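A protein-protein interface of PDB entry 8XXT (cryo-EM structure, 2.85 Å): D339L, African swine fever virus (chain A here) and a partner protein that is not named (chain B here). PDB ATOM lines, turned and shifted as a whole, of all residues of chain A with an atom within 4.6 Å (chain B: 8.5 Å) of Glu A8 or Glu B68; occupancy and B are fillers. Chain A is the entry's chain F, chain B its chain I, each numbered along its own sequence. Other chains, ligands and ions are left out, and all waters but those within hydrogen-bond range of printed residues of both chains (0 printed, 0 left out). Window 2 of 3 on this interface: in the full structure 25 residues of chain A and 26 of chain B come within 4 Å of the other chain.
Of the 18 printed residues of chain B, 7 touch a printed residue of chain A. Printed residues of chain B that touch a printed residue of chain A: Glu B68, Ile B69, Gly B70, Ser B71, Glu B145, Val B148 and Leu B152. Printed residues of chain A that touch a printed residue of chain B: Ile A6, Glu A8, Lys A41 and Arg A73. Hydrophobic or aromatic side chains of chain A within 4 Å of the printed part of chain B: Ile A6. Among the printed residues, no Asp or Glu carboxylate lies within 4 Å of a Lys or Arg side-chain nitrogen of the other chain.
No residue of chain B comes within 4 Å of Thr A9. Glu B68 touches just one residue of chain A: Glu A8 (3.3 Å). Of the printed residues of chain A, Gly B70 touches Lys A41 (3.7 Å). Of the printed residues of chain A, Glu B145 touches Ile A6. Printed residues of chain A within 4 Å of Leu B152: Arg A73 (3.6 Å). The nearest printed residue of chain A that does not touch Glu B145 is Phe A7 (8.1 Å).
The side-chain carboxylate (OE2) of Glu A8 lies within salt-bridge range of the guanidinium group (NH1) of Arg A73 (2.6 Å).
Among the printed residues, pairs that only touch across the chains: Ile A6 with Glu B145 (3.96 Å), Ile A6 with Val B148 (3.6 Å), Glu A8 with Glu B68 (3.3 Å), Lys A41 with Gly B70 (3.7 Å), Lys A41 with Ser B71 (3.1 Å) and Arg A73 with Leu B152 (3.6 Å).
The side-chain amino group (NZ) of Lys A41 sits close to the backbone carbonyl oxygen (O) of Ile B69, 2.4 Å away.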
ATOM      1  N   ILE A   6       9.078  -7.287   8.524  1.00  0.00           N
ATOM      2  CA  ILE A   6       8.020  -6.644   9.294  1.00  0.00           C
ATOM      3  C   ILE A   6       8.338  -5.162   9.423  1.00  0.00           C
ATOM      4  O   ILE A   6       9.419  -4.790   9.895  1.00  0.00           O
ATOM      5  CB  ILE A   6       7.865  -7.296  10.678  1.00  0.00           C
ATOM      6  CG1 ILE A   6       7.419  -8.748  10.529  1.00  0.00           C
ATOM      7  CG2 ILE A   6       6.874  -6.524  11.522  1.00  0.00           C
ATOM      8  CD1 ILE A   6       7.465  -9.524  11.814  1.00  0.00           C
ATOM      9  N   PHE A   7       7.398  -4.318   9.014  1.00  0.00           N
ATOM     10  CA  PHE A   7       7.570  -2.875   9.017  1.00  0.00           C
ATOM     11  C   PHE A   7       6.683  -2.227  10.070  1.00  0.00           C
ATOM     12  O   PHE A   7       5.742  -2.834  10.586  1.00  0.00           O
ATOM     13  CB  PHE A   7       7.231  -2.279   7.652  1.00  0.00           C
ATOM     14  CG  PHE A   7       8.184  -2.660   6.571  1.00  0.00           C
ATOM     15  CD1 PHE A   7       9.303  -1.893   6.315  1.00  0.00           C
ATOM     16  CD2 PHE A   7       7.954  -3.777   5.796  1.00  0.00           C
ATOM     17  CE1 PHE A   7      10.176  -2.238   5.314  1.00  0.00           C
ATOM     18  CE2 PHE A   7       8.825  -4.128   4.796  1.00  0.00           C
ATOM     19  CZ  PHE A   7       9.937  -3.355   4.553  1.00  0.00           C
ATOM     20  N   GLU A   8       6.999  -0.975  10.381  1.00  0.00           N
ATOM     21  CA  GLU A   8       6.167  -0.134  11.226  1.00  0.00           C
ATOM     22  C   GLU A   8       5.986   1.212  10.548  1.00  0.00           C
ATOM     23  O   GLU A   8       6.933   1.763   9.983  1.00  0.00           O
ATOM     24  CB  GLU A   8       6.777   0.065  12.613  1.00  0.00           C
ATOM     25  CG  GLU A   8       6.538  -1.079  13.570  1.00  0.00           C
ATOM     26  CD  GLU A   8       7.152  -0.826  14.929  1.00  0.00           C
ATOM     27  OE1 GLU A   8       7.573   0.318  15.188  1.00  0.00           O
ATOM     28  OE2 GLU A   8       7.218  -1.773  15.736  1.00  0.00           O
ATOM     29  N   THR A   9       4.770   1.738  10.603  1.00  0.00           N
ATOM     30  CA  THR A   9       4.487   3.010   9.962  1.00  0.00           C
ATOM     31  C   THR A   9       3.271   3.637  10.620  1.00  0.00           C
ATOM     32  O   THR A   9       2.498   2.968  11.309  1.00  0.00           O
ATOM     33  CB  THR A   9       4.255   2.840   8.460  1.00  0.00           C
ATOM     34  OG1 THR A   9       4.473   4.092   7.797  1.00  0.00           O
ATOM     35  CG2 THR A   9       2.839   2.371   8.183  1.00  0.00           C
ATOM     36  N   PHE A  40      11.938   1.027   1.082  1.00  0.00           N
ATOM     37  CA  PHE A  40      11.621   1.711   2.328  1.00  0.00           C
ATOM     38  C   PHE A  40      12.304   0.972   3.465  1.00  0.00           C
ATOM     39  O   PHE A  40      12.022  -0.208   3.692  1.00  0.00           O
ATOM     40  CB  PHE A  40      10.107   1.769   2.540  1.00  0.00           C
ATOM     41  CG  PHE A  40       9.698   2.169   3.929  1.00  0.00           C
ATOM     42  CD1 PHE A  40       9.927   3.451   4.391  1.00  0.00           C
ATOM     43  CD2 PHE A  40       9.073   1.262   4.769  1.00  0.00           C
ATOM     44  CE1 PHE A  40       9.546   3.818   5.664  1.00  0.00           C
ATOM     45  CE2 PHE A  40       8.691   1.624   6.042  1.00  0.00           C
ATOM     46  CZ  PHE A  40       8.928   2.901   6.489  1.00  0.00           C
ATOM     47  N   LYS A  41      13.203   1.661   4.166  1.00  0.00           N
ATOM     48  CA  LYS A  41      13.924   1.112   5.311  1.00  0.00           C
ATOM     49  C   LYS A  41      14.776  -0.096   4.910  1.00  0.00           C
ATOM     50  O   LYS A  41      14.614  -1.203   5.423  1.00  0.00           O
ATOM     51  CB  LYS A  41      12.962   0.756   6.447  1.00  0.00           C
ATOM     52  CG  LYS A  41      12.236   1.951   7.031  1.00  0.00           C
ATOM     53  CD  LYS A  41      11.962   1.780   8.517  1.00  0.00           C
ATOM     54  CE  LYS A  41      11.051   0.596   8.782  1.00  0.00           C
ATOM     55  NZ  LYS A  41      10.791   0.410  10.235  1.00  0.00           N
ATOM     56  N   VAL A  72       0.437   1.551  12.145  1.00  0.00           N
ATOM     57  CA  VAL A  72       0.306   0.231  11.542  1.00  0.00           C
ATOM     58  C   VAL A  72       1.625  -0.512  11.663  1.00  0.00           C
ATOM     59  O   VAL A  72       2.696   0.061  11.442  1.00  0.00           O
ATOM     60  CB  VAL A  72      -0.120   0.307  10.064  1.00  0.00           C
ATOM     61  CG1 VAL A  72      -0.792  -0.979   9.651  1.00  0.00           C
ATOM     62  CG2 VAL A  72      -1.044   1.480   9.838  1.00  0.00           C
ATOM     63  N   ARG A  73       1.545  -1.790  12.020  1.00  0.00           N
ATOM     64  CA  ARG A  73       2.670  -2.711  11.939  1.00  0.00           C
ATOM     65  C   ARG A  73       2.291  -3.816  10.967  1.00  0.00           C
ATOM     66  O   ARG A  73       1.292  -4.511  11.175  1.00  0.00           O
ATOM     67  CB  ARG A  73       3.016  -3.290  13.309  1.00  0.00           C
ATOM     68  CG  ARG A  73       3.912  -4.497  13.228  1.00  0.00           C
ATOM     69  CD  ARG A  73       5.005  -4.448  14.267  1.00  0.00           C
ATOM     70  NE  ARG A  73       4.501  -4.096  15.587  1.00  0.00           N
ATOM     71  CZ  ARG A  73       5.262  -3.977  16.665  1.00  0.00           C
ATOM     72  NH1 ARG A  73       6.571  -4.160  16.609  1.00  0.00           N
ATOM     73  NH2 ARG A  73       4.700  -3.664  17.829  1.00  0.00           N
ATOM     74  N   GLN B  61      17.463  -7.042  24.578  1.00  0.00           N
ATOM     75  CA  GLN B  61      16.506  -5.964  24.364  1.00  0.00           C
ATOM     76  C   GLN B  61      17.033  -4.936  23.374  1.00  0.00           C
ATOM     77  O   GLN B  61      16.248  -4.288  22.676  1.00  0.00           O
ATOM     78  CB  GLN B  61      16.163  -5.299  25.696  1.00  0.00           C
ATOM     79  CG  GLN B  61      16.033  -6.264  26.867  1.00  0.00           C
ATOM     80  CD  GLN B  61      14.857  -7.219  26.736  1.00  0.00           C
ATOM     81  OE1 GLN B  61      13.992  -7.052  25.877  1.00  0.00           O
ATOM     82  NE2 GLN B  61      14.823  -8.229  27.598  1.00  0.00           N
ATOM     83  N   CYS B  62      18.355  -4.785  23.281  1.00  0.00           N
ATOM     84  CA  CYS B  62      18.937  -3.855  22.319  1.00  0.00           C
ATOM     85  C   CYS B  62      18.714  -4.330  20.886  1.00  0.00           C
ATOM     86  O   CYS B  62      18.307  -3.550  20.008  1.00  0.00           O
ATOM     87  CB  CYS B  62      20.425  -3.687  22.616  1.00  0.00           C
ATOM     88  SG  CYS B  62      21.329  -2.723  21.414  1.00  0.00           S
ATOM     89  N   PHE B  63      18.979  -5.613  20.627  1.00  0.00           N
ATOM     90  CA  PHE B  63      18.681  -6.156  19.310  1.00  0.00           C
ATOM     91  C   PHE B  63      17.187  -6.112  19.036  1.00  0.00           C
ATOM     92  O   PHE B  63      16.772  -5.889  17.894  1.00  0.00           O
ATOM     93  CB  PHE B  63      19.192  -7.589  19.177  1.00  0.00           C
ATOM     94  CG  PHE B  63      18.875  -8.213  17.849  1.00  0.00           C
ATOM     95  CD1 PHE B  63      19.566  -7.832  16.713  1.00  0.00           C
ATOM     96  CD2 PHE B  63      17.858  -9.140  17.725  1.00  0.00           C
ATOM     97  CE1 PHE B  63      19.273  -8.391  15.487  1.00  0.00           C
ATOM     98  CE2 PHE B  63      17.559  -9.701  16.499  1.00  0.00           C
ATOM     99  CZ  PHE B  63      18.266  -9.324  15.380  1.00  0.00           C
ATOM    100  N   MET B  64      16.368  -6.322  20.069  1.00  0.00           N
ATOM    101  CA  MET B  64      14.926  -6.160  19.911  1.00  0.00           C
ATOM    102  C   MET B  64      14.579  -4.749  19.465  1.00  0.00           C
ATOM    103  O   MET B  64      13.740  -4.559  18.580  1.00  0.00           O
ATOM    104  CB  MET B  64      14.216  -6.497  21.219  1.00  0.00           C
ATOM    105  CG  MET B  64      13.694  -7.904  21.247  1.00  0.00           C
ATOM    106  SD  MET B  64      12.958  -8.311  19.659  1.00  0.00           S
ATOM    107  CE  MET B  64      13.927  -9.739  19.219  1.00  0.00           C
ATOM    108  N   ARG B  65      15.220  -3.749  20.067  1.00  0.00           N
ATOM    109  CA  ARG B  65      14.977  -2.364  19.685  1.00  0.00           C
ATOM    110  C   ARG B  65      15.305  -2.138  18.217  1.00  0.00           C
ATOM    111  O   ARG B  65      14.492  -1.587  17.464  1.00  0.00           O
ATOM    112  CB  ARG B  65      15.801  -1.428  20.567  1.00  0.00           C
ATOM    113  CG  ARG B  65      15.085  -0.976  21.819  1.00  0.00           C
ATOM    114  CD  ARG B  65      13.971   0.006  21.482  1.00  0.00           C
ATOM    115  NE  ARG B  65      14.396   1.404  21.455  1.00  0.00           N
ATOM    116  CZ  ARG B  65      15.009   2.046  22.442  1.00  0.00           C
ATOM    117  NH1 ARG B  65      15.242   1.471  23.610  1.00  0.00           N
ATOM    118  NH2 ARG B  65      15.378   3.311  22.259  1.00  0.00           N
ATOM    119  N   MET B  66      16.493  -2.565  17.784  1.00  0.00           N
ATOM    120  CA  MET B  66      16.871  -2.269  16.402  1.00  0.00           C
ATOM    121  C   MET B  66      16.055  -3.076  15.403  1.00  0.00           C
ATOM    122  O   MET B  66      15.811  -2.606  14.286  1.00  0.00           O
ATOM    123  CB  MET B  66      18.353  -2.509  16.161  1.00  0.00           C
ATOM    124  CG  MET B  66      18.934  -3.653  16.904  1.00  0.00           C
ATOM    125  SD  MET B  66      20.689  -3.369  17.077  1.00  0.00           S
ATOM    126  CE  MET B  66      21.100  -2.846  15.418  1.00  0.00           C
ATOM    127  N   ALA B  67      15.638  -4.290  15.767  1.00  0.00           N
ATOM    128  CA  ALA B  67      14.766  -5.052  14.884  1.00  0.00           C
ATOM    129  C   ALA B  67      13.375  -4.441  14.821  1.00  0.00           C
ATOM    130  O   ALA B  67      12.712  -4.510  13.780  1.00  0.00           O
ATOM    131  CB  ALA B  67      14.700  -6.505  15.346  1.00  0.00           C
ATOM    132  N   GLU B  68      12.916  -3.848  15.926  1.00  0.00           N
ATOM    133  CA  GLU B  68      11.667  -3.097  15.916  1.00  0.00           C
ATOM    134  C   GLU B  68      11.769  -1.888  14.999  1.00  0.00           C
ATOM    135  O   GLU B  68      10.828  -1.578  14.259  1.00  0.00           O
ATOM    136  CB  GLU B  68      11.317  -2.672  17.341  1.00  0.00           C
ATOM    137  CG  GLU B  68      10.015  -1.913  17.479  1.00  0.00           C
ATOM    138  CD  GLU B  68       9.705  -1.570  18.921  1.00  0.00           C
ATOM    139  OE1 GLU B  68       9.149  -2.431  19.634  1.00  0.00           O
ATOM    140  OE2 GLU B  68      10.028  -0.441  19.344  1.00  0.00           O
ATOM    141  N   ILE B  69      12.906  -1.190  15.037  1.00  0.00           N
ATOM    142  CA  ILE B  69      13.154  -0.123  14.072  1.00  0.00           C
ATOM    143  C   ILE B  69      13.160  -0.688  12.660  1.00  0.00           C
ATOM    144  O   ILE B  69      12.570  -0.112  11.740  1.00  0.00           O
ATOM    145  CB  ILE B  69      14.472   0.600  14.402  1.00  0.00           C
ATOM    146  CG1 ILE B  69      14.429   1.148  15.827  1.00  0.00           C
ATOM    147  CG2 ILE B  69      14.735   1.711  13.409  1.00  0.00           C
ATOM    148  CD1 ILE B  69      15.786   1.434  16.408  1.00  0.00           C
ATOM    149  N   GLY B  70      13.822  -1.826  12.470  1.00  0.00           N
ATOM    150  CA  GLY B  70      13.707  -2.573  11.233  1.00  0.00           C
ATOM    151  C   GLY B  70      14.284  -1.901  10.010  1.00  0.00           C
ATOM    152  O   GLY B  70      13.736  -2.052   8.914  1.00  0.00           O
ATOM    153  N   SER B  71      15.378  -1.160  10.163  1.00  0.00           N
ATOM    154  CA  SER B  71      16.037  -0.549   9.023  1.00  0.00           C
ATOM    155  C   SER B  71      17.555  -0.635   9.079  1.00  0.00           C
ATOM    156  O   SER B  71      18.216  -0.138   8.162  1.00  0.00           O
ATOM    157  CB  SER B  71      15.626   0.920   8.889  1.00  0.00           C
ATOM    158  OG  SER B  71      16.012   1.411   7.623  1.00  0.00           O
ATOM    159  N   PHE B  72      18.121  -1.238  10.118  1.00  0.00           N
ATOM    160  CA  PHE B  72      19.565  -1.369  10.209  1.00  0.00           C
ATOM    161  C   PHE B  72      20.083  -2.337   9.152  1.00  0.00           C
ATOM    162  O   PHE B  72      19.398  -3.281   8.750  1.00  0.00           O
ATOM    163  CB  PHE B  72      19.966  -1.845  11.602  1.00  0.00           C
ATOM    164  CG  PHE B  72      19.877  -0.781  12.653  1.00  0.00           C
ATOM    165  CD1 PHE B  72      18.679  -0.521  13.292  1.00  0.00           C
ATOM    166  CD2 PHE B  72      20.992  -0.042  13.005  1.00  0.00           C
ATOM    167  CE1 PHE B  72      18.595   0.456  14.260  1.00  0.00           C
ATOM    168  CE2 PHE B  72      20.912   0.937  13.974  1.00  0.00           C
ATOM    169  CZ  PHE B  72      19.712   1.185  14.602  1.00  0.00           C
ATOM    170  N   LEU B  77      23.341  -5.242  12.279  1.00  0.00           N
ATOM    171  CA  LEU B  77      22.445  -6.169  12.959  1.00  0.00           C
ATOM    172  C   LEU B  77      23.192  -7.411  13.421  1.00  0.00           C
ATOM    173  O   LEU B  77      23.018  -7.864  14.558  1.00  0.00           O
ATOM    174  CB  LEU B  77      21.288  -6.561  12.040  1.00  0.00           C
ATOM    175  CG  LEU B  77      20.074  -5.637  12.024  1.00  0.00           C
ATOM    176  CD1 LEU B  77      19.141  -6.020  10.889  1.00  0.00           C
ATOM    177  CD2 LEU B  77      19.350  -5.672  13.355  1.00  0.00           C
ATOM    178  N   ALA B 144      15.961 -11.793  13.128  1.00  0.00           N
ATOM    179  CA  ALA B 144      15.223 -10.616  13.572  1.00  0.00           C
ATOM    180  C   ALA B 144      13.725 -10.798  13.376  1.00  0.00           C
ATOM    181  O   ALA B 144      12.937 -10.600  14.312  1.00  0.00           O
ATOM    182  CB  ALA B 144      15.718  -9.379  12.823  1.00  0.00           C
ATOM    183  N   GLU B 145      13.310 -11.182  12.165  1.00  0.00           N
ATOM    184  CA  GLU B 145      11.885 -11.300  11.889  1.00  0.00           C
ATOM    185  C   GLU B 145      11.239 -12.324  12.808  1.00  0.00           C
ATOM    186  O   GLU B 145      10.173 -12.070  13.377  1.00  0.00           O
ATOM    187  CB  GLU B 145      11.656 -11.669  10.423  1.00  0.00           C
ATOM    188  CG  GLU B 145      10.186 -11.805  10.050  1.00  0.00           C
ATOM    189  CD  GLU B 145       9.974 -12.587   8.769  1.00  0.00           C
ATOM    190  OE1 GLU B 145      10.977 -12.986   8.144  1.00  0.00           O
ATOM    191  OE2 GLU B 145       8.805 -12.804   8.388  1.00  0.00           O
ATOM    192  N   VAL B 148      11.090 -11.025  16.631  1.00  0.00           N
ATOM    193  CA  VAL B 148      10.057 -10.010  16.832  1.00  0.00           C
ATOM    194  C   VAL B 148       8.669 -10.610  16.620  1.00  0.00           C
ATOM    195  O   VAL B 148       7.714 -10.254  17.323  1.00  0.00           O
ATOM    196  CB  VAL B 148      10.299  -8.762  15.958  1.00  0.00           C
ATOM    197  CG1 VAL B 148      11.758  -8.372  15.989  1.00  0.00           C
ATOM    198  CG2 VAL B 148       9.840  -8.980  14.526  1.00  0.00           C
ATOM    199  N   LYS B 151       7.856 -12.507  19.844  1.00  0.00           N
ATOM    200  CA  LYS B 151       7.580 -11.575  20.935  1.00  0.00           C
ATOM    201  C   LYS B 151       6.203 -10.948  20.787  1.00  0.00           C
ATOM    202  O   LYS B 151       5.464 -10.823  21.770  1.00  0.00           O
ATOM    203  CB  LYS B 151       8.652 -10.491  21.009  1.00  0.00           C
ATOM    204  CG  LYS B 151       8.908 -10.009  22.428  1.00  0.00           C
ATOM    205  CD  LYS B 151      10.240  -9.298  22.553  1.00  0.00           C
ATOM    206  CE  LYS B 151      11.286 -10.230  23.139  1.00  0.00           C
ATOM    207  NZ  LYS B 151      12.440  -9.492  23.716  1.00  0.00           N
ATOM    208  N   LEU B 152       5.835 -10.551  19.565  1.00  0.00           N
ATOM    209  CA  LEU B 152       4.496 -10.013  19.347  1.00  0.00           C
ATOM    210  C   LEU B 152       3.436 -11.068  19.628  1.00  0.00           C
ATOM    211  O   LEU B 152       2.393 -10.771  20.223  1.00  0.00           O
ATOM    212  CB  LEU B 152       4.368  -9.484  17.920  1.00  0.00           C
ATOM    213  CG  LEU B 152       5.220  -8.257  17.592  1.00  0.00           C
ATOM    214  CD1 LEU B 152       4.948  -7.765  16.176  1.00  0.00           C
ATOM    215  CD2 LEU B 152       4.997  -7.154  18.613  1.00  0.00           C
